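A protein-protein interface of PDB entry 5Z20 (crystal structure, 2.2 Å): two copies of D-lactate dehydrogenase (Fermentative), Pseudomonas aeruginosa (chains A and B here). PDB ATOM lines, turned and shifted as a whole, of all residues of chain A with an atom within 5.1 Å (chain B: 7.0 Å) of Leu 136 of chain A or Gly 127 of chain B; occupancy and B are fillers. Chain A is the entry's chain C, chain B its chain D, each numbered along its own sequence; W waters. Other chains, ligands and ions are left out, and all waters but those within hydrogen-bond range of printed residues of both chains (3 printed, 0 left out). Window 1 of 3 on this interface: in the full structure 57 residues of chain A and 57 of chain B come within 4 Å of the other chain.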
ATOM      1  N   LEU A 130     -14.763  -4.022  -1.579  1.00  0.00           N
ATOM      2  CA  LEU A 130     -15.078  -3.706  -2.966  1.00  0.00           C
ATOM      3  C   LEU A 130     -14.972  -4.866  -3.927  1.00  0.00           C
ATOM      4  O   LEU A 130     -15.759  -4.963  -4.902  1.00  0.00           O
ATOM      5  CB  LEU A 130     -14.215  -2.561  -3.442  1.00  0.00           C
ATOM      6  CG  LEU A 130     -14.709  -1.205  -2.893  1.00  0.00           C
ATOM      7  CD1 LEU A 130     -13.684  -0.115  -3.060  1.00  0.00           C
ATOM      8  CD2 LEU A 130     -15.995  -0.768  -3.598  1.00  0.00           C
ATOM      9  N   THR A 131     -14.014  -5.744  -3.694  1.00  0.00           N
ATOM     10  CA  THR A 131     -13.886  -6.944  -4.506  1.00  0.00           C
ATOM     11  C   THR A 131     -15.137  -7.804  -4.383  1.00  0.00           C
ATOM     12  O   THR A 131     -15.623  -8.282  -5.371  1.00  0.00           O
ATOM     13  CB  THR A 131     -12.646  -7.843  -4.099  1.00  0.00           C
ATOM     14  OG1 THR A 131     -11.483  -7.029  -4.155  1.00  0.00           O
ATOM     15  CG2 THR A 131     -12.483  -8.878  -5.098  1.00  0.00           C
ATOM     16  N   ARG A 134     -18.343  -5.739  -6.020  1.00  0.00           N
ATOM     17  CA  ARG A 134     -18.357  -5.701  -7.465  1.00  0.00           C
ATOM     18  C   ARG A 134     -17.906  -6.989  -8.162  1.00  0.00           C
ATOM     19  O   ARG A 134     -17.755  -7.027  -9.384  1.00  0.00           O
ATOM     20  CB  ARG A 134     -17.529  -4.508  -7.949  1.00  0.00           C
ATOM     21  CG  ARG A 134     -17.749  -3.256  -7.114  1.00  0.00           C
ATOM     22  CD  ARG A 134     -19.210  -2.841  -7.148  1.00  0.00           C
ATOM     23  NE  ARG A 134     -19.626  -2.480  -8.499  1.00  0.00           N
ATOM     24  CZ  ARG A 134     -19.808  -1.230  -8.910  1.00  0.00           C
ATOM     25  NH1 ARG A 134     -19.620  -0.221  -8.069  1.00  0.00           N
ATOM     26  NH2 ARG A 134     -20.181  -0.987 -10.159  1.00  0.00           N
ATOM     27  N   ARG A 135     -17.695  -8.028  -7.361  1.00  0.00           N
ATOM     28  CA  ARG A 135     -17.259  -9.322  -7.860  1.00  0.00           C
ATOM     29  C   ARG A 135     -16.033  -9.192  -8.741  1.00  0.00           C
ATOM     30  O   ARG A 135     -15.958  -9.798  -9.807  1.00  0.00           O
ATOM     31  CB  ARG A 135     -18.389 -10.013  -8.615  1.00  0.00           C
ATOM     32  CG  ARG A 135     -19.469 -10.544  -7.692  1.00  0.00           C
ATOM     33  CD  ARG A 135     -20.461  -9.454  -7.335  1.00  0.00           C
ATOM     34  NE  ARG A 135     -21.770 -10.016  -7.022  1.00  0.00           N
ATOM     35  CZ  ARG A 135     -22.561  -9.566  -6.059  1.00  0.00           C
ATOM     36  NH1 ARG A 135     -22.178  -8.540  -5.309  1.00  0.00           N
ATOM     37  NH2 ARG A 135     -23.739 -10.141  -5.844  1.00  0.00           N
ATOM     38  N   LEU A 136     -15.064  -8.405  -8.293  1.00  0.00           N
ATOM     39  CA  LEU A 136     -13.881  -8.120  -9.172  1.00  0.00           C
ATOM     40  C   LEU A 136     -12.964  -9.321  -9.402  1.00  0.00           C
ATOM     41  O   LEU A 136     -12.393  -9.457 -10.449  1.00  0.00           O
ATOM     42  CB  LEU A 136     -13.063  -7.000  -8.614  1.00  0.00           C
ATOM     43  CG  LEU A 136     -13.813  -5.654  -8.362  1.00  0.00           C
ATOM     44  CD1 LEU A 136     -12.886  -4.631  -7.669  1.00  0.00           C
ATOM     45  CD2 LEU A 136     -14.272  -5.100  -9.693  1.00  0.00           C
ATOM     46  N   HIS A 137     -12.886 -10.190  -8.410  1.00  0.00           N
ATOM     47  CA  HIS A 137     -12.140 -11.432  -8.491  1.00  0.00           C
ATOM     48  C   HIS A 137     -12.780 -12.385  -9.548  1.00  0.00           C
ATOM     49  O   HIS A 137     -12.047 -12.929 -10.390  1.00  0.00           O
ATOM     50  CB  HIS A 137     -12.058 -12.076  -7.121  1.00  0.00           C
ATOM     51  CG  HIS A 137     -13.373 -12.403  -6.500  1.00  0.00           C
ATOM     52  ND1 HIS A 137     -14.275 -11.451  -6.103  1.00  0.00           N
ATOM     53  CD2 HIS A 137     -13.917 -13.585  -6.158  1.00  0.00           C
ATOM     54  CE1 HIS A 137     -15.370 -12.028  -5.626  1.00  0.00           C
ATOM     55  NE2 HIS A 137     -15.160 -13.339  -5.605  1.00  0.00           N
ATOM     56  N   ARG A 138     -14.099 -12.384  -9.650  1.00  0.00           N
ATOM     57  CA  ARG A 138     -14.823 -13.185 -10.671  1.00  0.00           C
ATOM     58  C   ARG A 138     -14.742 -12.535 -12.036  1.00  0.00           C
ATOM     59  O   ARG A 138     -14.422 -13.195 -13.017  1.00  0.00           O
ATOM     60  CB  ARG A 138     -16.296 -13.431 -10.268  1.00  0.00           C
ATOM     61  CG  ARG A 138     -16.479 -14.036  -8.871  1.00  0.00           C
ATOM     62  CD  ARG A 138     -17.933 -14.461  -8.585  1.00  0.00           C
ATOM     63  NE  ARG A 138     -18.285 -15.444  -9.596  1.00  0.00           N
ATOM     64  CZ  ARG A 138     -19.500 -15.645 -10.086  1.00  0.00           C
ATOM     65  NH1 ARG A 138     -20.541 -14.887  -9.705  1.00  0.00           N
ATOM     66  NH2 ARG A 138     -19.662 -16.545 -11.032  1.00  0.00           N
ATOM     67  N   ALA A 139     -14.909 -11.197 -12.073  1.00  0.00           N
ATOM     68  CA  ALA A 139     -14.783 -10.464 -13.332  1.00  0.00           C
ATOM     69  C   ALA A 139     -13.456 -10.662 -13.976  1.00  0.00           C
ATOM     70  O   ALA A 139     -13.340 -10.880 -15.178  1.00  0.00           O
ATOM     71  CB  ALA A 139     -15.042  -8.960 -13.108  1.00  0.00           C
ATOM     72  N   TYR A 140     -12.437 -10.540 -13.175  1.00  0.00           N
ATOM     73  CA  TYR A 140     -11.068 -10.682 -13.684  1.00  0.00           C
ATOM     74  C   TYR A 140     -10.907 -12.000 -14.400  1.00  0.00           C
ATOM     75  O   TYR A 140     -10.378 -12.047 -15.525  1.00  0.00           O
ATOM     76  CB  TYR A 140     -10.052 -10.564 -12.547  1.00  0.00           C
ATOM     77  CG  TYR A 140      -8.635 -10.839 -12.969  1.00  0.00           C
ATOM     78  CD1 TYR A 140      -7.933  -9.903 -13.745  1.00  0.00           C
ATOM     79  CD2 TYR A 140      -8.018 -12.028 -12.642  1.00  0.00           C
ATOM     80  CE1 TYR A 140      -6.641 -10.126 -14.145  1.00  0.00           C
ATOM     81  CE2 TYR A 140      -6.720 -12.305 -13.074  1.00  0.00           C
ATOM     82  CZ  TYR A 140      -6.043 -11.342 -13.813  1.00  0.00           C
ATOM     83  OH  TYR A 140      -4.775 -11.550 -14.179  1.00  0.00           O
ATOM     84  N   ASN A 141     -11.290 -13.072 -13.761  1.00  0.00           N
ATOM     85  CA  ASN A 141     -11.145 -14.376 -14.351  1.00  0.00           C
ATOM     86  C   ASN A 141     -11.986 -14.511 -15.617  1.00  0.00           C
ATOM     87  O   ASN A 141     -11.581 -15.093 -16.540  1.00  0.00           O
ATOM     88  CB  ASN A 141     -11.369 -15.489 -13.345  1.00  0.00           C
ATOM     89  CG  ASN A 141     -10.268 -15.554 -12.309  1.00  0.00           C
ATOM     90  OD1 ASN A 141      -9.143 -15.230 -12.578  1.00  0.00           O
ATOM     91  ND2 ASN A 141     -10.613 -15.904 -11.156  1.00  0.00           N
ATOM     92  N   VAL B 121     -20.149   4.379 -10.075  1.00  0.00           N
ATOM     93  CA  VAL B 121     -19.022   4.431 -10.977  1.00  0.00           C
ATOM     94  C   VAL B 121     -17.734   4.807 -10.253  1.00  0.00           C
ATOM     95  O   VAL B 121     -16.731   4.145 -10.436  1.00  0.00           O
ATOM     96  CB  VAL B 121     -19.260   5.432 -12.121  1.00  0.00           C
ATOM     97  CG1 VAL B 121     -18.171   5.354 -13.142  1.00  0.00           C
ATOM     98  CG2 VAL B 121     -20.575   5.150 -12.818  1.00  0.00           C
ATOM     99  N   ALA B 122     -17.802   5.797  -9.376  1.00  0.00           N
ATOM    100  CA  ALA B 122     -16.659   6.176  -8.624  1.00  0.00           C
ATOM    101  C   ALA B 122     -16.173   5.065  -7.748  1.00  0.00           C
ATOM    102  O   ALA B 122     -14.953   4.821  -7.673  1.00  0.00           O
ATOM    103  CB  ALA B 122     -16.944   7.423  -7.780  1.00  0.00           C
ATOM    104  N   GLU B 123     -17.104   4.360  -7.088  1.00  0.00           N
ATOM    105  CA  GLU B 123     -16.719   3.247  -6.252  1.00  0.00           C
ATOM    106  C   GLU B 123     -15.992   2.165  -7.070  1.00  0.00           C
ATOM    107  O   GLU B 123     -15.073   1.478  -6.581  1.00  0.00           O
ATOM    108  CB  GLU B 123     -17.931   2.683  -5.541  1.00  0.00           C
ATOM    109  CG  GLU B 123     -18.470   3.685  -4.494  1.00  0.00           C
ATOM    110  CD  GLU B 123     -19.778   3.319  -3.837  1.00  0.00           C
ATOM    111  OE1 GLU B 123     -20.236   2.130  -3.964  1.00  0.00           O
ATOM    112  OE2 GLU B 123     -20.302   4.214  -3.071  1.00  0.00           O
ATOM    113  N   HIS B 124     -16.462   1.933  -8.277  1.00  0.00           N
ATOM    114  CA  HIS B 124     -15.887   0.850  -9.082  1.00  0.00           C
ATOM    115  C   HIS B 124     -14.472   1.241  -9.390  1.00  0.00           C
ATOM    116  O   HIS B 124     -13.578   0.399  -9.340  1.00  0.00           O
ATOM    117  CB  HIS B 124     -16.664   0.648 -10.369  1.00  0.00           C
ATOM    118  CG  HIS B 124     -16.242  -0.523 -11.153  1.00  0.00           C
ATOM    119  ND1 HIS B 124     -16.600  -1.799 -10.787  1.00  0.00           N
ATOM    120  CD2 HIS B 124     -15.467  -0.635 -12.259  1.00  0.00           C
ATOM    121  CE1 HIS B 124     -16.058  -2.662 -11.637  1.00  0.00           C
ATOM    122  NE2 HIS B 124     -15.375  -1.984 -12.548  1.00  0.00           N
ATOM    123  N   ALA B 125     -14.246   2.510  -9.737  1.00  0.00           N
ATOM    124  CA  ALA B 125     -12.898   2.970  -9.987  1.00  0.00           C
ATOM    125  C   ALA B 125     -12.011   2.730  -8.781  1.00  0.00           C
ATOM    126  O   ALA B 125     -10.844   2.323  -8.912  1.00  0.00           O
ATOM    127  CB  ALA B 125     -12.903   4.438 -10.367  1.00  0.00           C
ATOM    128  N   VAL B 126     -12.531   2.985  -7.579  1.00  0.00           N
ATOM    129  CA  VAL B 126     -11.746   2.752  -6.367  1.00  0.00           C
ATOM    130  C   VAL B 126     -11.485   1.278  -6.139  1.00  0.00           C
ATOM    131  O   VAL B 126     -10.364   0.868  -5.780  1.00  0.00           O
ATOM    132  CB  VAL B 126     -12.384   3.398  -5.141  1.00  0.00           C
ATOM    133  CG1 VAL B 126     -11.588   3.165  -3.864  1.00  0.00           C
ATOM    134  CG2 VAL B 126     -12.514   4.910  -5.339  1.00  0.00           C
ATOM    135  N   GLY B 127     -12.468   0.446  -6.409  1.00  0.00           N
ATOM    136  CA  GLY B 127     -12.255  -0.988  -6.449  1.00  0.00           C
ATOM    137  C   GLY B 127     -11.155  -1.456  -7.399  1.00  0.00           C
ATOM    138  O   GLY B 127     -10.343  -2.319  -7.037  1.00  0.00           O
ATOM    139  N   LEU B 128     -11.085  -0.885  -8.597  1.00  0.00           N
ATOM    140  CA  LEU B 128     -10.005  -1.260  -9.510  1.00  0.00           C
ATOM    141  C   LEU B 128      -8.645  -0.886  -8.886  1.00  0.00           C
ATOM    142  O   LEU B 128      -7.695  -1.675  -8.916  1.00  0.00           O
ATOM    143  CB  LEU B 128     -10.188  -0.610 -10.845  1.00  0.00           C
ATOM    144  CG  LEU B 128     -11.384  -1.099 -11.677  1.00  0.00           C
ATOM    145  CD1 LEU B 128     -11.512  -0.254 -12.902  1.00  0.00           C
ATOM    146  CD2 LEU B 128     -11.192  -2.537 -12.086  1.00  0.00           C
ATOM    147  N   ILE B 129      -8.574   0.321  -8.320  1.00  0.00           N
ATOM    148  CA  ILE B 129      -7.363   0.802  -7.692  1.00  0.00           C
ATOM    149  C   ILE B 129      -6.887  -0.193  -6.640  1.00  0.00           C
ATOM    150  O   ILE B 129      -5.732  -0.582  -6.611  1.00  0.00           O
ATOM    151  CB  ILE B 129      -7.557   2.205  -7.055  1.00  0.00           C
ATOM    152  CG1 ILE B 129      -7.628   3.260  -8.162  1.00  0.00           C
ATOM    153  CG2 ILE B 129      -6.384   2.533  -6.139  1.00  0.00           C
ATOM    154  CD1 ILE B 129      -8.076   4.652  -7.679  1.00  0.00           C
ATOM    155  N   LEU B 130      -7.763  -0.580  -5.759  1.00  0.00           N
ATOM    156  CA  LEU B 130      -7.369  -1.440  -4.680  1.00  0.00           C
ATOM    157  C   LEU B 130      -7.002  -2.852  -5.107  1.00  0.00           C
ATOM    158  O   LEU B 130      -6.110  -3.476  -4.486  1.00  0.00           O
ATOM    159  CB  LEU B 130      -8.431  -1.456  -3.596  1.00  0.00           C
ATOM    160  CG  LEU B 130      -8.383  -0.183  -2.703  1.00  0.00           C
ATOM    161  CD1 LEU B 130      -9.609  -0.046  -1.857  1.00  0.00           C
ATOM    162  CD2 LEU B 130      -7.200  -0.186  -1.766  1.00  0.00           C
ATOM    163  N   THR B 131      -7.740  -3.398  -6.082  1.00  0.00           N
ATOM    164  CA  THR B 131      -7.444  -4.703  -6.594  1.00  0.00           C
ATOM    165  C   THR B 131      -6.069  -4.716  -7.189  1.00  0.00           C
ATOM    166  O   THR B 131      -5.295  -5.608  -6.920  1.00  0.00           O
ATOM    167  CB  THR B 131      -8.410  -5.140  -7.686  1.00  0.00           C
ATOM    168  OG1 THR B 131      -9.744  -5.067  -7.178  1.00  0.00           O
ATOM    169  CG2 THR B 131      -8.149  -6.579  -7.975  1.00  0.00           C
ATOM    170  N   LEU B 132      -5.748  -3.705  -8.004  1.00  0.00           N
ATOM    171  CA  LEU B 132      -4.410  -3.577  -8.576  1.00  0.00           C
ATOM    172  C   LEU B 132      -3.348  -3.380  -7.534  1.00  0.00           C
ATOM    173  O   LEU B 132      -2.299  -4.059  -7.542  1.00  0.00           O
ATOM    174  CB  LEU B 132      -4.380  -2.409  -9.535  1.00  0.00           C
ATOM    175  CG  LEU B 132      -5.122  -2.649 -10.842  1.00  0.00           C
ATOM    176  CD1 LEU B 132      -5.414  -1.304 -11.551  1.00  0.00           C
ATOM    177  CD2 LEU B 132      -4.259  -3.536 -11.739  1.00  0.00           C
ATOM    178  N   ASN B 133      -3.638  -2.542  -6.558  1.00  0.00           N
ATOM    179  CA  ASN B 133      -2.642  -2.186  -5.514  1.00  0.00           C
ATOM    180  C   ASN B 133      -2.283  -3.401  -4.682  1.00  0.00           C
ATOM    181  O   ASN B 133      -1.118  -3.782  -4.560  1.00  0.00           O
ATOM    182  CB  ASN B 133      -3.200  -1.055  -4.695  1.00  0.00           C
ATOM    183  CG  ASN B 133      -2.267  -0.569  -3.578  1.00  0.00           C
ATOM    184  OD1 ASN B 133      -1.434  -1.271  -3.076  1.00  0.00           O
ATOM    185  ND2 ASN B 133      -2.514   0.649  -3.144  1.00  0.00           N
ATOM    186  N   LEU B 136      -5.370  -8.206  -5.417  1.00  0.00           N
ATOM    187  CA  LEU B 136      -6.421  -9.050  -4.851  1.00  0.00           C
ATOM    188  C   LEU B 136      -6.926 -10.122  -5.820  1.00  0.00           C
ATOM    189  O   LEU B 136      -7.299 -11.200  -5.433  1.00  0.00           O
ATOM    190  CB  LEU B 136      -7.626  -8.210  -4.408  1.00  0.00           C
ATOM    191  CG  LEU B 136      -7.331  -7.157  -3.341  1.00  0.00           C
ATOM    192  CD1 LEU B 136      -8.567  -6.312  -3.010  1.00  0.00           C
ATOM    193  CD2 LEU B 136      -6.815  -7.811  -2.074  1.00  0.00           C
ATOM    194  N   HIS B 137      -6.901  -9.785  -7.081  1.00  0.00           N
ATOM    195  CA  HIS B 137      -7.282 -10.724  -8.183  1.00  0.00           C
ATOM    196  C   HIS B 137      -6.267 -11.891  -8.212  1.00  0.00           C
ATOM    197  O   HIS B 137      -6.691 -13.038  -8.310  1.00  0.00           O
ATOM    198  CB  HIS B 137      -7.380  -9.992  -9.525  1.00  0.00           C
ATOM    199  CG  HIS B 137      -6.143  -9.297  -9.955  1.00  0.00           C
ATOM    200  ND1 HIS B 137      -5.618  -8.222  -9.276  1.00  0.00           N
ATOM    201  CD2 HIS B 137      -5.350  -9.470 -11.037  1.00  0.00           C
ATOM    202  CE1 HIS B 137      -4.517  -7.798  -9.887  1.00  0.00           C
ATOM    203  NE2 HIS B 137      -4.350  -8.525 -10.982  1.00  0.00           N
ATOM    204  N   PHE B 175     -15.528  10.608  -6.947  1.00  0.00           N
ATOM    205  CA  PHE B 175     -14.283   9.851  -6.870  1.00  0.00           C
ATOM    206  C   PHE B 175     -13.237  10.606  -6.037  1.00  0.00           C
ATOM    207  O   PHE B 175     -12.618  10.063  -5.093  1.00  0.00           O
ATOM    208  CB  PHE B 175     -13.765   9.595  -8.236  1.00  0.00           C
ATOM    209  CG  PHE B 175     -12.408   8.975  -8.255  1.00  0.00           C
ATOM    210  CD1 PHE B 175     -12.244   7.606  -8.028  1.00  0.00           C
ATOM    211  CD2 PHE B 175     -11.298   9.725  -8.545  1.00  0.00           C
ATOM    212  CE1 PHE B 175     -10.994   7.024  -8.063  1.00  0.00           C
ATOM    213  CE2 PHE B 175     -10.023   9.166  -8.534  1.00  0.00           C
ATOM    214  CZ  PHE B 175      -9.857   7.809  -8.300  1.00  0.00           C
ATOM    215  N   ILE B 246      -6.304   4.624 -14.347  1.00  0.00           N
ATOM    216  CA  ILE B 246      -7.639   4.046 -14.267  1.00  0.00           C
ATOM    217  C   ILE B 246      -8.506   4.729 -15.325  1.00  0.00           C
ATOM    218  O   ILE B 246      -8.624   5.973 -15.351  1.00  0.00           O
ATOM    219  CB  ILE B 246      -8.307   4.299 -12.896  1.00  0.00           C
ATOM    220  CG1 ILE B 246      -7.445   3.741 -11.735  1.00  0.00           C
ATOM    221  CG2 ILE B 246      -9.679   3.667 -12.839  1.00  0.00           C
ATOM    222  CD1 ILE B 246      -7.197   2.220 -11.774  1.00  0.00           C
ATOM    223  N   VAL B 307      -6.065  -4.939 -14.890  1.00  0.00           N
ATOM    224  CA  VAL B 307      -7.391  -5.558 -14.645  1.00  0.00           C
ATOM    225  C   VAL B 307      -8.381  -4.881 -15.568  1.00  0.00           C
ATOM    226  O   VAL B 307      -8.486  -3.629 -15.604  1.00  0.00           O
ATOM    227  CB  VAL B 307      -7.808  -5.338 -13.187  1.00  0.00           C
ATOM    228  CG1 VAL B 307      -9.255  -5.761 -12.986  1.00  0.00           C
ATOM    229  CG2 VAL B 307      -6.931  -6.136 -12.274  1.00  0.00           C
ATOM    230  N   VAL B 308      -9.119  -5.688 -16.295  1.00  0.00           N
ATOM    231  CA  VAL B 308     -10.187  -5.259 -17.110  1.00  0.00           C
ATOM    232  C   VAL B 308     -11.505  -5.811 -16.603  1.00  0.00           C
ATOM    233  O   VAL B 308     -11.688  -6.994 -16.487  1.00  0.00           O
ATOM    234  CB  VAL B 308      -9.989  -5.760 -18.560  1.00  0.00           C
ATOM    235  CG1 VAL B 308     -11.106  -5.291 -19.454  1.00  0.00           C
ATOM    236  CG2 VAL B 308      -8.672  -5.258 -19.148  1.00  0.00           C
ATOM    237  N   THR B 309     -12.450  -4.932 -16.351  1.00  0.00           N
ATOM    238  CA  THR B 309     -13.821  -5.331 -16.125  1.00  0.00           C
ATOM    239  C   THR B 309     -14.612  -4.844 -17.355  1.00  0.00           C
ATOM    240  O   THR B 309     -14.274  -3.828 -17.992  1.00  0.00           O
ATOM    241  CB  THR B 309     -14.398  -4.710 -14.862  1.00  0.00           C
ATOM    242  OG1 THR B 309     -14.223  -3.302 -14.861  1.00  0.00           O
ATOM    243  CG2 THR B 309     -13.715  -5.264 -13.691  1.00  0.00           C
ATOM    244  N   GLN B 312     -18.814  -2.588 -16.391  1.00  0.00           N
ATOM    245  CA  GLN B 312     -19.730  -2.846 -15.299  1.00  0.00           C
ATOM    246  C   GLN B 312     -19.652  -1.775 -14.196  1.00  0.00           C
ATOM    247  O   GLN B 312     -20.224  -1.984 -13.114  1.00  0.00           O
ATOM    248  CB  GLN B 312     -19.462  -4.204 -14.654  1.00  0.00           C
ATOM    249  CG  GLN B 312     -18.123  -4.381 -14.058  1.00  0.00           C
ATOM    250  CD  GLN B 312     -17.969  -5.689 -13.299  1.00  0.00           C
ATOM    251  OE1 GLN B 312     -17.420  -6.649 -13.830  1.00  0.00           O
ATOM    252  NE2 GLN B 312     -18.405  -5.709 -12.012  1.00  0.00           N
HETATM  253  O   HOH W   1     -20.739  -4.568 -10.307  1.00  0.00           O
HETATM  254  O   HOH W   2      -9.327 -13.241  -9.623  1.00  0.00           O
HETATM  255  O   HOH W   3     -20.194  -0.007  -5.305  1.00  0.00           O
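Thr 131 of chain A touches Leu 136 of chain B, and with the chains exchanged Leu 136 of chain A touches Thr 131 of chain B.
Positions printed for both chains: 130, 131, 136 and 137.
The backbone carbonyl oxygen of Arg 134 of chain A lies within hydrogen-bond range of the side-chain amide nitrogen of Gln 312 of chain B (3.0 Å).
Leu 136 of chain A touches just these residues of chain B: His 124 (3.6 Å), Gly 127 (3.5 Å) and Thr 131 (3.2 Å).
Gly 127 of chain B touches just these residues of chain A: Leu 130 (3.6 Å) and Leu 136 (3.5 Å).
Printed residues of chain B within 4 Å of Thr 131 of chain A: Leu 136 (3.2 Å).
Printed residues of chain A within 4 Å of Val 126 of chain B: Leu 130.
Printed residues of chain A within 4 Å of Leu 136 of chain B: Thr 131 (3.2 Å).
Of the printed residues of chain B, Arg 134 of chain A touches His 124 and Gln 312.
Printed residues of chain B within 4 Å of Tyr 140 of chain A: His 137 (3.4 Å).
CG1 of Val 126 of chain B touches CD1 of Leu 130 of chain A (3.97 Å).
N of Gly 127 of chain B touches CD1 of Leu 130 of chain A (3.6 Å).
CD1 of Leu 136 of chain B touches OG1 of Thr 131 of chain A, at 3.2 Å.
ND1 of His 124 of chain B touches NH2 of Arg 134 of chain A (3.7 Å).
His 124 of chain B touches Leu 136 of chain A (CE1 to CD2, 3.6 Å).
Leu 136 of chain A touches Gly 127 of chain B (CD1 to O, 3.5 Å).
CD1 of Leu 136 of chain A touches OG1 of Thr 131 of chain B (3.2 Å).
Ala 139 of chain A touches Thr 309 of chain B.
CB of Ala 139 of chain A touches OE1 of Gln 312 of chain B (3.4 Å).
CZ of Tyr 140 of chain A touches CD2 of His 137 of chain B (3.4 Å).
The backbone NH of Leu 136 of chain B lies within hydrogen-bond range of the backbone carbonyl oxygen of Thr 131 of chain B, at 3.0 Å.
N of Leu 136 of chain A is in hydrogen-bond range of O of Thr 131 of chain A, at 3.0 Å.
OG1 of Thr 309 of chain B sits at hydrogen-bond distance from NE2 of His 124 of chain B.
The backbone carbonyl oxygen (O) of Gly 127 of chain B lies within hydrogen-bond range of the side-chain hydroxyl (OG1) of Thr 131 of chain B, 2.8 Å away.
Hydrophobic or aromatic side chains of chain A within 4 Å of the printed part of chain B: Leu 130, Leu 136, Ala 139 and Tyr 140.
Along chain A the printed residues that touch a printed residue of chain B span positions 130 to 140.
Among the printed residues, 12 pairs touch across the chains.
Water W3 lies within hydrogen-bond range of OE1 of Glu 123 of chain B and NH1 of Arg 134 of chain A.
Water W2 lies within hydrogen-bond range of O of His 137 of chain A (2.8 Å), O of His 137 of chain B (3.0 Å) and ND2 of Asn 141 of chain A (3.3 Å).
Water W1 lies within hydrogen-bond range of the guanidinium group of Arg 134 of chain A (3.0 Å) and the side-chain amide nitrogen of Gln 312 of chain B (3.1 Å).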
